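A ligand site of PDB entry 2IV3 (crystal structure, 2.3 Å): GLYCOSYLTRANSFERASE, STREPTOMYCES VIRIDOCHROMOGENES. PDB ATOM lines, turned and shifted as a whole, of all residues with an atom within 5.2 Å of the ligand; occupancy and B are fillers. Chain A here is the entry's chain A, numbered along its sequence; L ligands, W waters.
The side-chain hydroxyl (OH) of Tyr 29 sits at hydrogen-bond distance from an oxygen (O12) of the ligand (2.6 Å). O7 of the ligand sits close to N of Thr 256 (3.2 Å). O2 of the ligand lies within hydrogen-bond range of N of Val 220 (2.9 Å). N of Gly 30 lies within hydrogen-bond range of O4 of the ligand. The backbone carbonyl oxygen (O) of Val 220 lies within hydrogen-bond range of a nitrogen (N2) of the ligand, at 2.7 Å. An oxygen (O10) of the ligand is in salt-bridge range of the side-chain amino group of Lys 175, at 3.7 Å. An oxygen (O8) of the ligand sits at hydrogen-bond distance from the backbone NH (N) of Val 257. An oxygen (O3) of the ligand lies within hydrogen-bond range of the guanidinium group (NH2) of Arg 225 (2.9 Å). The backbone NH of Gly 195 sits close to an oxygen (O2) of the ligand (3.4 Å). The side-chain carboxylate (OE1) of Glu 260 sits at hydrogen-bond distance from an oxygen (O3) of the ligand, 2.6 Å away.
The backbone carbonyl oxygen (O) of Gly 218 lies within hydrogen-bond range of the backbone NH (N) of Gly 195 (2.8 Å). OE2 of Glu 219 lies within hydrogen-bond range of N of Tyr 29 (2.9 Å). The guanidinium group (NH2) of Arg 225 is in salt-bridge range of the side-chain carboxylate (OE2) of Glu 260 (2.8 Å). OE2 of Glu 260 is in hydrogen-bond range of OG1 of Thr 256, 3.1 Å away. The side-chain carboxylate (OE1) of Glu 252 lies within hydrogen-bond range of the indole nitrogen (NE1) of Trp 250, at 3.0 Å. The backbone carbonyl oxygen of Gly 195 lies within hydrogen-bond range of the backbone NH of Glu 219 (3.4 Å). NZ of Lys 175 is in salt-bridge range of OE2 of Glu 252 (3.2 Å). The side-chain hydroxyl (OH) of Tyr 29 sits at hydrogen-bond distance from the guanidinium group (NH1) of Arg 170 (3.3 Å).
The backbone carbonyl oxygen (O) of Gly 28 sits close to an oxygen (O1) of the ligand, at 3.2 Å. Residues that only touch the ligand: Trp 34 (3.4 Å), Glu 219 (3.5 Å), Met 168 (3.5 Å), Gly 169 (3.7 Å), Gly 31 (3.7 Å), Ala 194 (3.7 Å) and Glu 252 (3.8 Å). Of the 24 residues printed, 17 come within 4 Å of the ligand. The nearest printed residue that does not touch the ligand is Ala 255 (4.04 Å).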
ATOM      1  N   GLY A  28       2.748  17.242   4.037  1.00  0.00           N
ATOM      2  CA  GLY A  28       2.458  18.593   3.615  1.00  0.00           C
ATOM      3  C   GLY A  28       1.044  18.927   4.034  1.00  0.00           C
ATOM      4  O   GLY A  28       0.652  18.639   5.200  1.00  0.00           O
ATOM      5  N   TYR A  29       0.302  19.511   3.085  1.00  0.00           N
ATOM      6  CA  TYR A  29      -1.087  19.972   3.284  1.00  0.00           C
ATOM      7  C   TYR A  29      -2.015  18.823   3.541  1.00  0.00           C
ATOM      8  O   TYR A  29      -1.953  17.836   2.870  1.00  0.00           O
ATOM      9  CB  TYR A  29      -1.563  20.759   2.066  1.00  0.00           C
ATOM     10  CG  TYR A  29      -3.049  20.978   1.981  1.00  0.00           C
ATOM     11  CD1 TYR A  29      -3.639  22.125   2.515  1.00  0.00           C
ATOM     12  CD2 TYR A  29      -3.876  20.045   1.341  1.00  0.00           C
ATOM     13  CE1 TYR A  29      -5.024  22.341   2.435  1.00  0.00           C
ATOM     14  CE2 TYR A  29      -5.250  20.243   1.263  1.00  0.00           C
ATOM     15  CZ  TYR A  29      -5.804  21.391   1.798  1.00  0.00           C
ATOM     16  OH  TYR A  29      -7.161  21.579   1.689  1.00  0.00           O
ATOM     17  N   GLY A  30      -2.879  18.955   4.528  1.00  0.00           N
ATOM     18  CA  GLY A  30      -3.933  17.981   4.775  1.00  0.00           C
ATOM     19  C   GLY A  30      -4.301  18.063   6.252  1.00  0.00           C
ATOM     20  O   GLY A  30      -3.429  17.844   7.094  1.00  0.00           O
ATOM     21  N   GLY A  31      -5.566  18.368   6.547  1.00  0.00           N
ATOM     22  CA  GLY A  31      -6.024  18.595   7.937  1.00  0.00           C
ATOM     23  C   GLY A  31      -6.800  17.472   8.592  1.00  0.00           C
ATOM     24  O   GLY A  31      -6.873  17.380   9.834  1.00  0.00           O
ATOM     25  N   TRP A  34      -3.934  15.467  10.010  1.00  0.00           N
ATOM     26  CA  TRP A  34      -3.547  16.040  11.306  1.00  0.00           C
ATOM     27  C   TRP A  34      -4.579  15.766  12.429  1.00  0.00           C
ATOM     28  O   TRP A  34      -4.230  15.291  13.521  1.00  0.00           O
ATOM     29  CB  TRP A  34      -3.253  17.553  11.155  1.00  0.00           C
ATOM     30  CG  TRP A  34      -1.822  17.847  10.779  1.00  0.00           C
ATOM     31  CD1 TRP A  34      -1.363  18.441   9.636  1.00  0.00           C
ATOM     32  CD2 TRP A  34      -0.645  17.538  11.561  1.00  0.00           C
ATOM     33  NE1 TRP A  34       0.012  18.493   9.640  1.00  0.00           N
ATOM     34  CE2 TRP A  34       0.474  17.992  10.830  1.00  0.00           C
ATOM     35  CE3 TRP A  34      -0.443  16.941  12.815  1.00  0.00           C
ATOM     36  CZ2 TRP A  34       1.788  17.845  11.294  1.00  0.00           C
ATOM     37  CZ3 TRP A  34       0.857  16.807  13.293  1.00  0.00           C
ATOM     38  CH2 TRP A  34       1.957  17.258  12.539  1.00  0.00           C
ATOM     39  N   MET A 168      -2.216  29.776   5.887  1.00  0.00           N
ATOM     40  CA  MET A 168      -1.795  28.403   5.742  1.00  0.00           C
ATOM     41  C   MET A 168      -2.932  27.482   5.322  1.00  0.00           C
ATOM     42  O   MET A 168      -3.605  26.868   6.162  1.00  0.00           O
ATOM     43  CB  MET A 168      -1.063  27.907   7.012  1.00  0.00           C
ATOM     44  CG  MET A 168      -0.553  26.503   6.868  1.00  0.00           C
ATOM     45  SD  MET A 168       1.191  26.211   7.203  1.00  0.00           S
ATOM     46  CE  MET A 168       2.014  27.732   6.714  1.00  0.00           C
ATOM     47  N   GLY A 169      -3.137  27.379   4.017  1.00  0.00           N
ATOM     48  CA  GLY A 169      -4.169  26.449   3.508  1.00  0.00           C
ATOM     49  C   GLY A 169      -4.168  26.394   1.998  1.00  0.00           C
ATOM     50  O   GLY A 169      -3.223  26.904   1.333  1.00  0.00           O
ATOM     51  N   ARG A 170      -5.205  25.773   1.419  1.00  0.00           N
ATOM     52  CA  ARG A 170      -5.361  25.881  -0.043  1.00  0.00           C
ATOM     53  C   ARG A 170      -5.749  27.299  -0.467  1.00  0.00           C
ATOM     54  O   ARG A 170      -6.696  27.896   0.068  1.00  0.00           O
ATOM     55  CB  ARG A 170      -6.258  24.825  -0.666  1.00  0.00           C
ATOM     56  CG  ARG A 170      -5.491  23.709  -1.356  1.00  0.00           C
ATOM     57  CD  ARG A 170      -6.223  23.138  -2.601  1.00  0.00           C
ATOM     58  NE  ARG A 170      -7.178  22.059  -2.284  1.00  0.00           N
ATOM     59  CZ  ARG A 170      -8.214  22.166  -1.434  1.00  0.00           C
ATOM     60  NH1 ARG A 170      -8.446  23.311  -0.787  1.00  0.00           N
ATOM     61  NH2 ARG A 170      -9.010  21.103  -1.213  1.00  0.00           N
ATOM     62  N   LYS A 175     -11.521  29.773   1.086  1.00  0.00           N
ATOM     63  CA  LYS A 175     -10.621  29.818   2.256  1.00  0.00           C
ATOM     64  C   LYS A 175     -10.274  31.265   2.494  1.00  0.00           C
ATOM     65  O   LYS A 175      -9.726  31.626   3.554  1.00  0.00           O
ATOM     66  CB  LYS A 175      -9.349  28.983   2.059  1.00  0.00           C
ATOM     67  CG  LYS A 175      -9.519  27.461   1.706  1.00  0.00           C
ATOM     68  CD  LYS A 175     -10.300  26.678   2.744  1.00  0.00           C
ATOM     69  CE  LYS A 175      -9.732  26.867   4.171  1.00  0.00           C
ATOM     70  NZ  LYS A 175     -10.767  26.428   5.204  1.00  0.00           N
ATOM     71  N   ALA A 194       1.218  30.674   2.595  1.00  0.00           N
ATOM     72  CA  ALA A 194       1.751  29.322   2.551  1.00  0.00           C
ATOM     73  C   ALA A 194       0.677  28.335   2.132  1.00  0.00           C
ATOM     74  O   ALA A 194      -0.411  28.339   2.670  1.00  0.00           O
ATOM     75  CB  ALA A 194       2.385  28.957   3.882  1.00  0.00           C
ATOM     76  N   GLY A 195       0.943  27.505   1.125  1.00  0.00           N
ATOM     77  CA  GLY A 195      -0.095  26.577   0.663  1.00  0.00           C
ATOM     78  C   GLY A 195      -0.117  26.275  -0.824  1.00  0.00           C
ATOM     79  O   GLY A 195       0.490  27.017  -1.624  1.00  0.00           O
ATOM     80  N   PRO A 196      -0.809  25.177  -1.198  1.00  0.00           N
ATOM     81  CA  PRO A 196      -1.085  24.831  -2.597  1.00  0.00           C
ATOM     82  C   PRO A 196      -1.876  25.940  -3.291  1.00  0.00           C
ATOM     83  O   PRO A 196      -2.928  26.375  -2.787  1.00  0.00           O
ATOM     84  CB  PRO A 196      -1.950  23.567  -2.501  1.00  0.00           C
ATOM     85  CG  PRO A 196      -1.731  23.021  -1.161  1.00  0.00           C
ATOM     86  CD  PRO A 196      -1.361  24.174  -0.263  1.00  0.00           C
ATOM     87  N   GLY A 218       4.232  28.622  -1.510  1.00  0.00           N
ATOM     88  CA  GLY A 218       3.748  27.307  -1.939  1.00  0.00           C
ATOM     89  C   GLY A 218       3.527  26.419  -0.730  1.00  0.00           C
ATOM     90  O   GLY A 218       3.592  26.895   0.403  1.00  0.00           O
ATOM     91  N   GLU A 219       3.262  25.140  -0.980  1.00  0.00           N
ATOM     92  CA  GLU A 219       3.006  24.173   0.087  1.00  0.00           C
ATOM     93  C   GLU A 219       4.187  24.063   1.043  1.00  0.00           C
ATOM     94  O   GLU A 219       5.337  24.158   0.621  1.00  0.00           O
ATOM     95  CB  GLU A 219       2.709  22.794  -0.514  1.00  0.00           C
ATOM     96  CG  GLU A 219       1.843  21.928   0.433  1.00  0.00           C
ATOM     97  CD  GLU A 219       1.259  20.658  -0.221  1.00  0.00           C
ATOM     98  OE1 GLU A 219       0.654  20.748  -1.307  1.00  0.00           O
ATOM     99  OE2 GLU A 219       1.365  19.568   0.387  1.00  0.00           O
ATOM    100  N   VAL A 220       3.909  23.867   2.320  1.00  0.00           N
ATOM    101  CA  VAL A 220       4.962  23.630   3.293  1.00  0.00           C
ATOM    102  C   VAL A 220       4.628  22.497   4.232  1.00  0.00           C
ATOM    103  O   VAL A 220       3.449  22.123   4.425  1.00  0.00           O
ATOM    104  CB  VAL A 220       5.368  24.934   4.129  1.00  0.00           C
ATOM    105  CG1 VAL A 220       6.071  26.021   3.235  1.00  0.00           C
ATOM    106  CG2 VAL A 220       4.204  25.494   4.897  1.00  0.00           C
ATOM    107  N   GLY A 221       5.691  21.961   4.829  1.00  0.00           N
ATOM    108  CA  GLY A 221       5.587  20.942   5.840  1.00  0.00           C
ATOM    109  C   GLY A 221       6.748  20.964   6.810  1.00  0.00           C
ATOM    110  O   GLY A 221       7.538  21.892   6.814  1.00  0.00           O
ATOM    111  N   ARG A 225       6.967  24.440   8.324  1.00  0.00           N
ATOM    112  CA  ARG A 225       5.563  24.614   8.762  1.00  0.00           C
ATOM    113  C   ARG A 225       5.443  25.069  10.230  1.00  0.00           C
ATOM    114  O   ARG A 225       4.855  26.113  10.530  1.00  0.00           O
ATOM    115  CB  ARG A 225       4.726  23.386   8.481  1.00  0.00           C
ATOM    116  CG  ARG A 225       3.272  23.606   8.697  1.00  0.00           C
ATOM    117  CD  ARG A 225       2.619  22.251   8.679  1.00  0.00           C
ATOM    118  NE  ARG A 225       1.262  22.141   9.232  1.00  0.00           N
ATOM    119  CZ  ARG A 225       0.990  21.587  10.414  1.00  0.00           C
ATOM    120  NH1 ARG A 225       1.999  21.213  11.201  1.00  0.00           N
ATOM    121  NH2 ARG A 225      -0.273  21.462  10.843  1.00  0.00           N
ATOM    122  N   LEU A 229       4.054  28.688  11.737  1.00  0.00           N
ATOM    123  CA  LEU A 229       2.982  28.732  12.683  1.00  0.00           C
ATOM    124  C   LEU A 229       3.433  29.470  13.944  1.00  0.00           C
ATOM    125  O   LEU A 229       2.646  30.185  14.534  1.00  0.00           O
ATOM    126  CB  LEU A 229       2.539  27.313  13.021  1.00  0.00           C
ATOM    127  CG  LEU A 229       1.215  26.657  12.558  1.00  0.00           C
ATOM    128  CD1 LEU A 229       0.389  27.421  11.560  1.00  0.00           C
ATOM    129  CD2 LEU A 229       1.436  25.230  12.072  1.00  0.00           C
ATOM    130  N   TRP A 250     -20.323  27.647   1.267  1.00  0.00           N
ATOM    131  CA  TRP A 250     -19.241  27.094   2.078  1.00  0.00           C
ATOM    132  C   TRP A 250     -19.442  27.403   3.565  1.00  0.00           C
ATOM    133  O   TRP A 250     -19.910  28.473   3.962  1.00  0.00           O
ATOM    134  CB  TRP A 250     -17.876  27.559   1.560  1.00  0.00           C
ATOM    135  CG  TRP A 250     -16.730  27.074   2.446  1.00  0.00           C
ATOM    136  CD1 TRP A 250     -16.077  27.803   3.371  1.00  0.00           C
ATOM    137  CD2 TRP A 250     -16.175  25.761   2.485  1.00  0.00           C
ATOM    138  NE1 TRP A 250     -15.154  27.025   4.008  1.00  0.00           N
ATOM    139  CE2 TRP A 250     -15.177  25.766   3.476  1.00  0.00           C
ATOM    140  CE3 TRP A 250     -16.424  24.578   1.790  1.00  0.00           C
ATOM    141  CZ2 TRP A 250     -14.416  24.638   3.783  1.00  0.00           C
ATOM    142  CZ3 TRP A 250     -15.661  23.461   2.088  1.00  0.00           C
ATOM    143  CH2 TRP A 250     -14.681  23.497   3.079  1.00  0.00           C
ATOM    144  N   GLU A 252     -17.313  26.468   7.058  1.00  0.00           N
ATOM    145  CA  GLU A 252     -16.084  25.900   7.510  1.00  0.00           C
ATOM    146  C   GLU A 252     -16.442  24.973   8.682  1.00  0.00           C
ATOM    147  O   GLU A 252     -17.005  25.418   9.681  1.00  0.00           O
ATOM    148  CB  GLU A 252     -15.120  27.025   7.872  1.00  0.00           C
ATOM    149  CG  GLU A 252     -13.724  26.618   8.208  1.00  0.00           C
ATOM    150  CD  GLU A 252     -13.046  25.939   7.075  1.00  0.00           C
ATOM    151  OE1 GLU A 252     -12.968  26.546   5.998  1.00  0.00           O
ATOM    152  OE2 GLU A 252     -12.580  24.804   7.266  1.00  0.00           O
ATOM    153  N   ALA A 255     -11.900  23.786  10.738  1.00  0.00           N
ATOM    154  CA  ALA A 255     -10.836  24.802  10.673  1.00  0.00           C
ATOM    155  C   ALA A 255      -9.590  24.371  11.459  1.00  0.00           C
ATOM    156  O   ALA A 255      -9.243  24.935  12.511  1.00  0.00           O
ATOM    157  CB  ALA A 255     -11.381  26.186  11.168  1.00  0.00           C
ATOM    158  N   THR A 256      -8.903  23.346  10.974  1.00  0.00           N
ATOM    159  CA  THR A 256      -7.776  22.797  11.721  1.00  0.00           C
ATOM    160  C   THR A 256      -6.631  23.791  12.049  1.00  0.00           C
ATOM    161  O   THR A 256      -6.001  23.661  13.116  1.00  0.00           O
ATOM    162  CB  THR A 256      -7.275  21.447  11.161  1.00  0.00           C
ATOM    163  OG1 THR A 256      -6.002  21.086  11.772  1.00  0.00           O
ATOM    164  CG2 THR A 256      -7.119  21.530   9.716  1.00  0.00           C
ATOM    165  N   VAL A 257      -6.387  24.763  11.178  1.00  0.00           N
ATOM    166  CA  VAL A 257      -5.278  25.724  11.368  1.00  0.00           C
ATOM    167  C   VAL A 257      -5.408  26.619  12.605  1.00  0.00           C
ATOM    168  O   VAL A 257      -4.420  27.136  13.123  1.00  0.00           O
ATOM    169  CB  VAL A 257      -5.064  26.647  10.132  1.00  0.00           C
ATOM    170  CG1 VAL A 257      -6.237  27.549   9.932  1.00  0.00           C
ATOM    171  CG2 VAL A 257      -3.872  27.492  10.336  1.00  0.00           C
ATOM    172  N   GLU A 260      -3.838  24.884  15.530  1.00  0.00           N
ATOM    173  CA  GLU A 260      -2.393  24.852  15.249  1.00  0.00           C
ATOM    174  C   GLU A 260      -1.708  26.137  15.595  1.00  0.00           C
ATOM    175  O   GLU A 260      -0.759  26.139  16.361  1.00  0.00           O
ATOM    176  CB  GLU A 260      -2.123  24.504  13.793  1.00  0.00           C
ATOM    177  CG  GLU A 260      -2.602  23.138  13.490  1.00  0.00           C
ATOM    178  CD  GLU A 260      -2.651  22.841  11.998  1.00  0.00           C
ATOM    179  OE1 GLU A 260      -2.358  23.737  11.173  1.00  0.00           O
ATOM    180  OE2 GLU A 260      -2.981  21.680  11.658  1.00  0.00           O
HETATM  181  N1  LIG L   1      -1.163  22.935   5.548  1.00  0.00           N
HETATM  182  C1  LIG L   1       0.192  22.551   5.466  1.00  0.00           C
HETATM  183  N2  LIG L   1       0.995  23.193   4.597  1.00  0.00           N
HETATM  184  C2  LIG L   1       0.536  24.172   3.823  1.00  0.00           C
HETATM  185  C3  LIG L   1      -0.783  24.580   3.877  1.00  0.00           C
HETATM  186  C4  LIG L   1      -1.628  23.920   4.770  1.00  0.00           C
HETATM  187  O1  LIG L   1       0.628  21.627   6.197  1.00  0.00           O
HETATM  188  O2  LIG L   1       1.290  24.760   3.056  1.00  0.00           O
HETATM  189  C5  LIG L   1      -2.069  22.237   6.480  1.00  0.00           C
HETATM  190  C6  LIG L   1      -2.543  23.030   7.709  1.00  0.00           C
HETATM  191  O3  LIG L   1      -1.664  23.064   8.811  1.00  0.00           O
HETATM  192  C7  LIG L   1      -3.773  22.247   8.120  1.00  0.00           C
HETATM  193  C8  LIG L   1      -4.363  21.864   6.763  1.00  0.00           C
HETATM  194  O4  LIG L   1      -3.294  21.984   5.794  1.00  0.00           O
HETATM  195  O5  LIG L   1      -3.371  21.107   8.888  1.00  0.00           O
HETATM  196  C9  LIG L   1      -5.412  22.886   6.402  1.00  0.00           C
HETATM  197  O6  LIG L   1      -6.644  22.348   6.817  1.00  0.00           O
HETATM  198  P1  LIG L   1      -7.901  23.289   7.173  1.00  0.00           P
HETATM  199  O7  LIG L   1      -9.029  22.485   7.878  1.00  0.00           O
HETATM  200  O8  LIG L   1      -7.547  24.552   7.974  1.00  0.00           O
HETATM  201  O9  LIG L   1      -8.434  23.766   5.736  1.00  0.00           O
HETATM  202  P2  LIG L   1      -9.086  22.715   4.691  1.00  0.00           P
HETATM  203  O10 LIG L   1     -10.628  22.769   4.752  1.00  0.00           O
HETATM  204  O11 LIG L   1      -8.563  21.202   5.079  1.00  0.00           O
HETATM  205  O12 LIG L   1      -8.545  23.030   3.296  1.00  0.00           O
HETATM  206  O   HOH W   1     -13.458  21.872   5.486  1.00  0.00           O
